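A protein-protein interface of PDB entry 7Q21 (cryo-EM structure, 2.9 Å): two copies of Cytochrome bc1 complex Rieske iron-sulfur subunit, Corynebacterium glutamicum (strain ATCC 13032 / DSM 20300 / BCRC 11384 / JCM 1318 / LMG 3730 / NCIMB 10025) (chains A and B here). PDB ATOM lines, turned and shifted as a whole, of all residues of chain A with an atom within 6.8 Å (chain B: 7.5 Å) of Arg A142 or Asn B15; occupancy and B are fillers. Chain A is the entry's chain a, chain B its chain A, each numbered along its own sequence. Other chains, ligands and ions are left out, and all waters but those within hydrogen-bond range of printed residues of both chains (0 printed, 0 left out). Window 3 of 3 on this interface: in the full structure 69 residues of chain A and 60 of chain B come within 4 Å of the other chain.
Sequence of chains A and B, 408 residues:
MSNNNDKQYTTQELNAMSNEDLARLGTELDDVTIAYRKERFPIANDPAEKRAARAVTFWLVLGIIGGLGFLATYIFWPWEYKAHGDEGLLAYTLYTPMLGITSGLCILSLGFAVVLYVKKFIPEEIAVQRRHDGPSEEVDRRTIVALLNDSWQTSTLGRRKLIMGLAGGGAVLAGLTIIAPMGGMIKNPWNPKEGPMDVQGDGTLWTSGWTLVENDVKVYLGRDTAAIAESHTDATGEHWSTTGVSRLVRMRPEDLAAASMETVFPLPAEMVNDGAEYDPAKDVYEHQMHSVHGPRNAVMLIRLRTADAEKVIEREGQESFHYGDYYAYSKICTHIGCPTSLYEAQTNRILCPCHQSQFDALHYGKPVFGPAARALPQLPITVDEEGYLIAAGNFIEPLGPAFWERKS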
ATOM      1  N   GLU A 137     -10.041  25.762 -12.912  1.00  0.00           N
ATOM      2  CA  GLU A 137      -9.737  24.645 -13.788  1.00  0.00           C
ATOM      3  C   GLU A 137     -10.804  23.564 -13.626  1.00  0.00           C
ATOM      4  O   GLU A 137     -11.576  23.592 -12.674  1.00  0.00           O
ATOM      5  CB  GLU A 137      -8.326  24.115 -13.506  1.00  0.00           C
ATOM      6  CG  GLU A 137      -7.634  23.550 -14.735  1.00  0.00           C
ATOM      7  CD  GLU A 137      -7.732  24.356 -16.023  1.00  0.00           C
ATOM      8  OE1 GLU A 137      -7.505  25.586 -15.982  1.00  0.00           O
ATOM      9  OE2 GLU A 137      -8.031  23.747 -17.071  1.00  0.00           O
ATOM     10  N   GLU A 138     -10.865  22.651 -14.603  1.00  0.00           N
ATOM     11  CA  GLU A 138     -11.786  21.530 -14.594  1.00  0.00           C
ATOM     12  C   GLU A 138     -11.386  20.498 -13.540  1.00  0.00           C
ATOM     13  O   GLU A 138     -12.242  19.769 -13.040  1.00  0.00           O
ATOM     14  CB  GLU A 138     -11.937  20.937 -16.002  1.00  0.00           C
ATOM     15  CG  GLU A 138     -13.093  19.949 -16.138  1.00  0.00           C
ATOM     16  CD  GLU A 138     -14.388  20.315 -15.424  1.00  0.00           C
ATOM     17  OE1 GLU A 138     -14.784  21.502 -15.499  1.00  0.00           O
ATOM     18  OE2 GLU A 138     -14.995  19.418 -14.794  1.00  0.00           O
ATOM     19  N   VAL A 139     -10.076  20.419 -13.258  1.00  0.00           N
ATOM     20  CA  VAL A 139      -9.486  19.460 -12.334  1.00  0.00           C
ATOM     21  C   VAL A 139      -9.571  19.978 -10.900  1.00  0.00           C
ATOM     22  O   VAL A 139      -9.888  19.205  -9.995  1.00  0.00           O
ATOM     23  CB  VAL A 139      -8.045  19.052 -12.724  1.00  0.00           C
ATOM     24  CG1 VAL A 139      -7.076  20.221 -12.733  1.00  0.00           C
ATOM     25  CG2 VAL A 139      -7.508  17.932 -11.845  1.00  0.00           C
ATOM     26  N   ASP A 140      -9.330  21.281 -10.703  1.00  0.00           N
ATOM     27  CA  ASP A 140      -9.255  21.865  -9.369  1.00  0.00           C
ATOM     28  C   ASP A 140     -10.625  21.907  -8.697  1.00  0.00           C
ATOM     29  O   ASP A 140     -10.738  21.622  -7.507  1.00  0.00           O
ATOM     30  CB  ASP A 140      -8.565  23.226  -9.367  1.00  0.00           C
ATOM     31  CG  ASP A 140      -7.098  23.151  -9.753  1.00  0.00           C
ATOM     32  OD1 ASP A 140      -6.343  22.394  -9.101  1.00  0.00           O
ATOM     33  OD2 ASP A 140      -6.712  23.868 -10.692  1.00  0.00           O
ATOM     34  N   ARG A 141     -11.658  22.210  -9.491  1.00  0.00           N
ATOM     35  CA  ARG A 141     -13.043  22.219  -9.043  1.00  0.00           C
ATOM     36  C   ARG A 141     -13.459  20.837  -8.558  1.00  0.00           C
ATOM     37  O   ARG A 141     -14.062  20.729  -7.496  1.00  0.00           O
ATOM     38  CB  ARG A 141     -13.972  22.664 -10.177  1.00  0.00           C
ATOM     39  CG  ARG A 141     -14.239  24.160 -10.200  1.00  0.00           C
ATOM     40  CD  ARG A 141     -14.826  24.610 -11.522  1.00  0.00           C
ATOM     41  NE  ARG A 141     -16.281  24.581 -11.552  1.00  0.00           N
ATOM     42  CZ  ARG A 141     -17.073  25.631 -11.349  1.00  0.00           C
ATOM     43  NH1 ARG A 141     -16.562  26.823 -11.091  1.00  0.00           N
ATOM     44  NH2 ARG A 141     -18.385  25.484 -11.405  1.00  0.00           N
ATOM     45  N   ARG A 142     -13.127  19.786  -9.321  1.00  0.00           N
ATOM     46  CA  ARG A 142     -13.584  18.429  -9.058  1.00  0.00           C
ATOM     47  C   ARG A 142     -12.915  17.882  -7.796  1.00  0.00           C
ATOM     48  O   ARG A 142     -13.553  17.199  -7.000  1.00  0.00           O
ATOM     49  CB  ARG A 142     -13.292  17.514 -10.254  1.00  0.00           C
ATOM     50  CG  ARG A 142     -14.009  17.886 -11.542  1.00  0.00           C
ATOM     51  CD  ARG A 142     -15.515  17.726 -11.500  1.00  0.00           C
ATOM     52  NE  ARG A 142     -15.901  16.327 -11.351  1.00  0.00           N
ATOM     53  CZ  ARG A 142     -15.972  15.437 -12.338  1.00  0.00           C
ATOM     54  NH1 ARG A 142     -15.689  15.785 -13.583  1.00  0.00           N
ATOM     55  NH2 ARG A 142     -16.334  14.194 -12.071  1.00  0.00           N
ATOM     56  N   THR A 143     -11.669  18.311  -7.562  1.00  0.00           N
ATOM     57  CA  THR A 143     -10.841  17.754  -6.505  1.00  0.00           C
ATOM     58  C   THR A 143     -10.941  18.582  -5.222  1.00  0.00           C
ATOM     59  O   THR A 143     -10.364  18.188  -4.212  1.00  0.00           O
ATOM     60  CB  THR A 143      -9.399  17.550  -6.983  1.00  0.00           C
ATOM     61  OG1 THR A 143      -8.820  18.840  -7.166  1.00  0.00           O
ATOM     62  CG2 THR A 143      -9.259  16.716  -8.240  1.00  0.00           C
ATOM     63  N   ILE A 144     -11.689  19.694  -5.255  1.00  0.00           N
ATOM     64  CA  ILE A 144     -11.964  20.448  -4.039  1.00  0.00           C
ATOM     65  C   ILE A 144     -13.312  20.026  -3.472  1.00  0.00           C
ATOM     66  O   ILE A 144     -13.475  20.007  -2.259  1.00  0.00           O
ATOM     67  CB  ILE A 144     -11.839  21.983  -4.199  1.00  0.00           C
ATOM     68  CG1 ILE A 144     -11.889  22.720  -2.858  1.00  0.00           C
ATOM     69  CG2 ILE A 144     -12.898  22.541  -5.133  1.00  0.00           C
ATOM     70  CD1 ILE A 144     -10.768  22.404  -1.910  1.00  0.00           C
ATOM     71  N   VAL A 145     -14.263  19.683  -4.343  1.00  0.00           N
ATOM     72  CA  VAL A 145     -15.565  19.227  -3.892  1.00  0.00           C
ATOM     73  C   VAL A 145     -15.462  17.769  -3.453  1.00  0.00           C
ATOM     74  O   VAL A 145     -16.340  17.311  -2.744  1.00  0.00           O
ATOM     75  CB  VAL A 145     -16.695  19.453  -4.919  1.00  0.00           C
ATOM     76  CG1 VAL A 145     -16.970  20.923  -5.197  1.00  0.00           C
ATOM     77  CG2 VAL A 145     -16.525  18.675  -6.214  1.00  0.00           C
ATOM     78  N   ALA A 146     -14.431  17.065  -3.936  1.00  0.00           N
ATOM     79  CA  ALA A 146     -14.196  15.677  -3.566  1.00  0.00           C
ATOM     80  C   ALA A 146     -13.464  15.604  -2.229  1.00  0.00           C
ATOM     81  O   ALA A 146     -13.699  14.681  -1.458  1.00  0.00           O
ATOM     82  CB  ALA A 146     -13.442  14.956  -4.657  1.00  0.00           C
ATOM     83  N   LEU A 147     -12.546  16.547  -1.984  1.00  0.00           N
ATOM     84  CA  LEU A 147     -11.820  16.602  -0.726  1.00  0.00           C
ATOM     85  C   LEU A 147     -12.741  17.047   0.409  1.00  0.00           C
ATOM     86  O   LEU A 147     -12.707  16.457   1.490  1.00  0.00           O
ATOM     87  CB  LEU A 147     -10.590  17.504  -0.853  1.00  0.00           C
ATOM     88  CG  LEU A 147      -9.328  16.814  -1.364  1.00  0.00           C
ATOM     89  CD1 LEU A 147      -8.179  17.801  -1.447  1.00  0.00           C
ATOM     90  CD2 LEU A 147      -8.941  15.642  -0.473  1.00  0.00           C
ATOM     91  N   THR B  10      -8.245  15.477 -19.270  1.00  0.00           N
ATOM     92  CA  THR B  10      -9.413  15.758 -20.086  1.00  0.00           C
ATOM     93  C   THR B  10     -10.674  15.759 -19.222  1.00  0.00           C
ATOM     94  O   THR B  10     -10.633  15.481 -18.020  1.00  0.00           O
ATOM     95  CB  THR B  10      -9.537  14.763 -21.249  1.00  0.00           C
ATOM     96  OG1 THR B  10      -9.971  13.505 -20.731  1.00  0.00           O
ATOM     97  CG2 THR B  10      -8.252  14.580 -22.024  1.00  0.00           C
ATOM     98  N   THR B  11     -11.791  16.136 -19.855  1.00  0.00           N
ATOM     99  CA  THR B  11     -13.083  16.274 -19.195  1.00  0.00           C
ATOM    100  C   THR B  11     -13.778  14.915 -19.105  1.00  0.00           C
ATOM    101  O   THR B  11     -14.498  14.663 -18.138  1.00  0.00           O
ATOM    102  CB  THR B  11     -13.946  17.358 -19.859  1.00  0.00           C
ATOM    103  OG1 THR B  11     -13.121  18.511 -20.032  1.00  0.00           O
ATOM    104  CG2 THR B  11     -15.173  17.723 -19.054  1.00  0.00           C
ATOM    105  N   GLN B  12     -13.565  14.061 -20.119  1.00  0.00           N
ATOM    106  CA  GLN B  12     -14.195  12.750 -20.177  1.00  0.00           C
ATOM    107  C   GLN B  12     -13.465  11.743 -19.290  1.00  0.00           C
ATOM    108  O   GLN B  12     -13.922  10.612 -19.185  1.00  0.00           O
ATOM    109  CB  GLN B  12     -14.375  12.278 -21.625  1.00  0.00           C
ATOM    110  CG  GLN B  12     -13.090  11.851 -22.324  1.00  0.00           C
ATOM    111  CD  GLN B  12     -12.730  10.390 -22.197  1.00  0.00           C
ATOM    112  OE1 GLN B  12     -13.590   9.512 -22.121  1.00  0.00           O
ATOM    113  NE2 GLN B  12     -11.436  10.114 -22.180  1.00  0.00           N
ATOM    114  N   GLU B  13     -12.320  12.126 -18.713  1.00  0.00           N
ATOM    115  CA  GLU B  13     -11.488  11.230 -17.918  1.00  0.00           C
ATOM    116  C   GLU B  13     -11.742  11.472 -16.428  1.00  0.00           C
ATOM    117  O   GLU B  13     -11.734  10.529 -15.625  1.00  0.00           O
ATOM    118  CB  GLU B  13     -10.024  11.261 -18.386  1.00  0.00           C
ATOM    119  CG  GLU B  13      -8.985  11.129 -17.287  1.00  0.00           C
ATOM    120  CD  GLU B  13      -7.553  11.420 -17.699  1.00  0.00           C
ATOM    121  OE1 GLU B  13      -7.335  12.067 -18.751  1.00  0.00           O
ATOM    122  OE2 GLU B  13      -6.648  10.992 -16.964  1.00  0.00           O
ATOM    123  N   LEU B  14     -11.990  12.738 -16.052  1.00  0.00           N
ATOM    124  CA  LEU B  14     -12.167  13.102 -14.653  1.00  0.00           C
ATOM    125  C   LEU B  14     -13.455  12.498 -14.091  1.00  0.00           C
ATOM    126  O   LEU B  14     -13.478  12.067 -12.940  1.00  0.00           O
ATOM    127  CB  LEU B  14     -12.158  14.627 -14.503  1.00  0.00           C
ATOM    128  CG  LEU B  14     -10.786  15.296 -14.418  1.00  0.00           C
ATOM    129  CD1 LEU B  14     -10.837  16.719 -14.957  1.00  0.00           C
ATOM    130  CD2 LEU B  14     -10.275  15.296 -12.989  1.00  0.00           C
ATOM    131  N   ASN B  15     -14.500  12.448 -14.920  1.00  0.00           N
ATOM    132  CA  ASN B  15     -15.775  11.869 -14.528  1.00  0.00           C
ATOM    133  C   ASN B  15     -15.697  10.344 -14.541  1.00  0.00           C
ATOM    134  O   ASN B  15     -16.629   9.686 -14.081  1.00  0.00           O
ATOM    135  CB  ASN B  15     -16.929  12.383 -15.392  1.00  0.00           C
ATOM    136  CG  ASN B  15     -16.584  12.427 -16.864  1.00  0.00           C
ATOM    137  OD1 ASN B  15     -15.843  11.583 -17.362  1.00  0.00           O
ATOM    138  ND2 ASN B  15     -17.103  13.421 -17.565  1.00  0.00           N
ATOM    139  N   ALA B  16     -14.598   9.793 -15.076  1.00  0.00           N
ATOM    140  CA  ALA B  16     -14.384   8.352 -15.123  1.00  0.00           C
ATOM    141  C   ALA B  16     -13.587   7.869 -13.908  1.00  0.00           C
ATOM    142  O   ALA B  16     -13.143   6.725 -13.873  1.00  0.00           O
ATOM    143  CB  ALA B  16     -13.726   7.963 -16.426  1.00  0.00           C
ATOM    144  N   MET B  17     -13.432   8.746 -12.904  1.00  0.00           N
ATOM    145  CA  MET B  17     -12.728   8.416 -11.674  1.00  0.00           C
ATOM    146  C   MET B  17     -13.693   8.497 -10.493  1.00  0.00           C
ATOM    147  O   MET B  17     -14.547   9.385 -10.449  1.00  0.00           O
ATOM    148  CB  MET B  17     -11.561   9.378 -11.441  1.00  0.00           C
ATOM    149  CG  MET B  17     -10.447   9.220 -12.451  1.00  0.00           C
ATOM    150  SD  MET B  17      -9.000  10.181 -11.978  1.00  0.00           S
ATOM    151  CE  MET B  17      -9.540  11.824 -12.442  1.00  0.00           C
ATOM    152  N   SER B  18     -13.525   7.578  -9.534  1.00  0.00           N
ATOM    153  CA  SER B  18     -14.322   7.551  -8.311  1.00  0.00           C
ATOM    154  C   SER B  18     -14.060   8.802  -7.477  1.00  0.00           C
ATOM    155  O   SER B  18     -13.066   9.494  -7.704  1.00  0.00           O
ATOM    156  CB  SER B  18     -14.066   6.305  -7.508  1.00  0.00           C
ATOM    157  OG  SER B  18     -12.679   6.148  -7.264  1.00  0.00           O
ATOM    158  N   ASN B  19     -14.979   9.090  -6.546  1.00  0.00           N
ATOM    159  CA  ASN B  19     -14.898  10.276  -5.704  1.00  0.00           C
ATOM    160  C   ASN B  19     -13.655  10.197  -4.818  1.00  0.00           C
ATOM    161  O   ASN B  19     -13.001  11.214  -4.571  1.00  0.00           O
ATOM    162  CB  ASN B  19     -16.223  10.557  -4.983  1.00  0.00           C
ATOM    163  CG  ASN B  19     -16.134  11.368  -3.705  1.00  0.00           C
ATOM    164  OD1 ASN B  19     -15.470  12.404  -3.640  1.00  0.00           O
ATOM    165  ND2 ASN B  19     -16.801  10.891  -2.670  1.00  0.00           N
ATOM    166  N   LEU B  22     -10.634  10.991  -6.876  1.00  0.00           N
ATOM    167  CA  LEU B  22     -10.533  12.435  -7.003  1.00  0.00           C
ATOM    168  C   LEU B  22      -9.918  13.024  -5.737  1.00  0.00           C
ATOM    169  O   LEU B  22      -9.099  13.941  -5.828  1.00  0.00           O
ATOM    170  CB  LEU B  22     -11.904  13.046  -7.305  1.00  0.00           C
ATOM    171  CG  LEU B  22     -12.365  12.956  -8.758  1.00  0.00           C
ATOM    172  CD1 LEU B  22     -13.755  13.553  -8.915  1.00  0.00           C
ATOM    173  CD2 LEU B  22     -11.380  13.641  -9.693  1.00  0.00           C
ATOM    174  N   ALA B  23     -10.290  12.465  -4.574  1.00  0.00           N
ATOM    175  CA  ALA B  23      -9.762  12.909  -3.294  1.00  0.00           C
ATOM    176  C   ALA B  23      -8.267  12.615  -3.209  1.00  0.00           C
ATOM    177  O   ALA B  23      -7.515  13.450  -2.727  1.00  0.00           O
ATOM    178  CB  ALA B  23     -10.525  12.290  -2.150  1.00  0.00           C
ATOM    179  N   GLY B  26      -6.407  15.075  -5.603  1.00  0.00           N
ATOM    180  CA  GLY B  26      -6.406  16.448  -5.118  1.00  0.00           C
ATOM    181  C   GLY B  26      -5.337  16.679  -4.054  1.00  0.00           C
ATOM    182  O   GLY B  26      -4.621  17.676  -4.097  1.00  0.00           O
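The guanidinium group (NH1) of Arg A142 is in salt-bridge range of the side-chain carboxylate (OE2) of Glu A138, at 3.9 Å.
The backbone carbonyl oxygen of Gln B12 lies close to the side-chain amide oxygen of Asn B15, at 2.8 Å.
The backbone carbonyl oxygen of Thr B11 sits at hydrogen-bond distance from the side-chain amide nitrogen of Asn B15, 2.9 Å away.
The side-chain hydroxyl (OG1) of Thr A143 sits at hydrogen-bond distance from the backbone carbonyl oxygen (O) of Asp A140, 3.4 Å away.
O of Val A139 sits at hydrogen-bond distance from OG1 of Thr A143 (3.0 Å).
Among the printed residues, merely in contact across the chains: Ala A146 with Asn B19, Arg A142 with Asn B15, Leu A147 with Ala B23, Ala A146 with Leu B22, Arg A142 with Leu B14, Thr A143 with Leu B22, Thr A143 with Gly B26, Glu A138 with Leu B14 and Val A139 with Leu B14.
Printed residues of chain B within 4 Å of Val A139: Leu B14.
Arg A142 touches just these residues of chain B: Leu B14 and Asn B15.
Printed residues of chain B within 4 Å of Ala A146: Asn B19 and Leu B22.
Gln B12 touches none of the printed residues of chain A.
Of chain A, only Arg A142 comes within 4 Å of Asn B15.
Of the printed residues of chain A, Leu B22 touches Thr A143 and Ala A146.
Of the printed residues of chain A, Ala B23 touches Leu A147.
Of the printed residues of chain A, Gly B26 touches Thr A143 (3.7 Å).
The nearest residue of chain B that does not touch Arg A142 is Leu B22 (4.1 Å).
The nearest printed residue of chain B that does not touch Val A139 is Leu B22 (5.8 Å).
Hydrophobic or aromatic side chains of chain B that line the printed part of chain A: Leu B14 and Leu B22.
Hydrophobic or aromatic side chains of chain A that line the printed part of chain B: Val A139, Ala A146 and Leu A147.
Among the printed residues, 9 pairs touch across the chains.
Among the printed residues, no Asp or Glu carboxylate lies within 4 Å of a Lys or Arg side-chain nitrogen of the other chain.
No position is printed for both chains.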
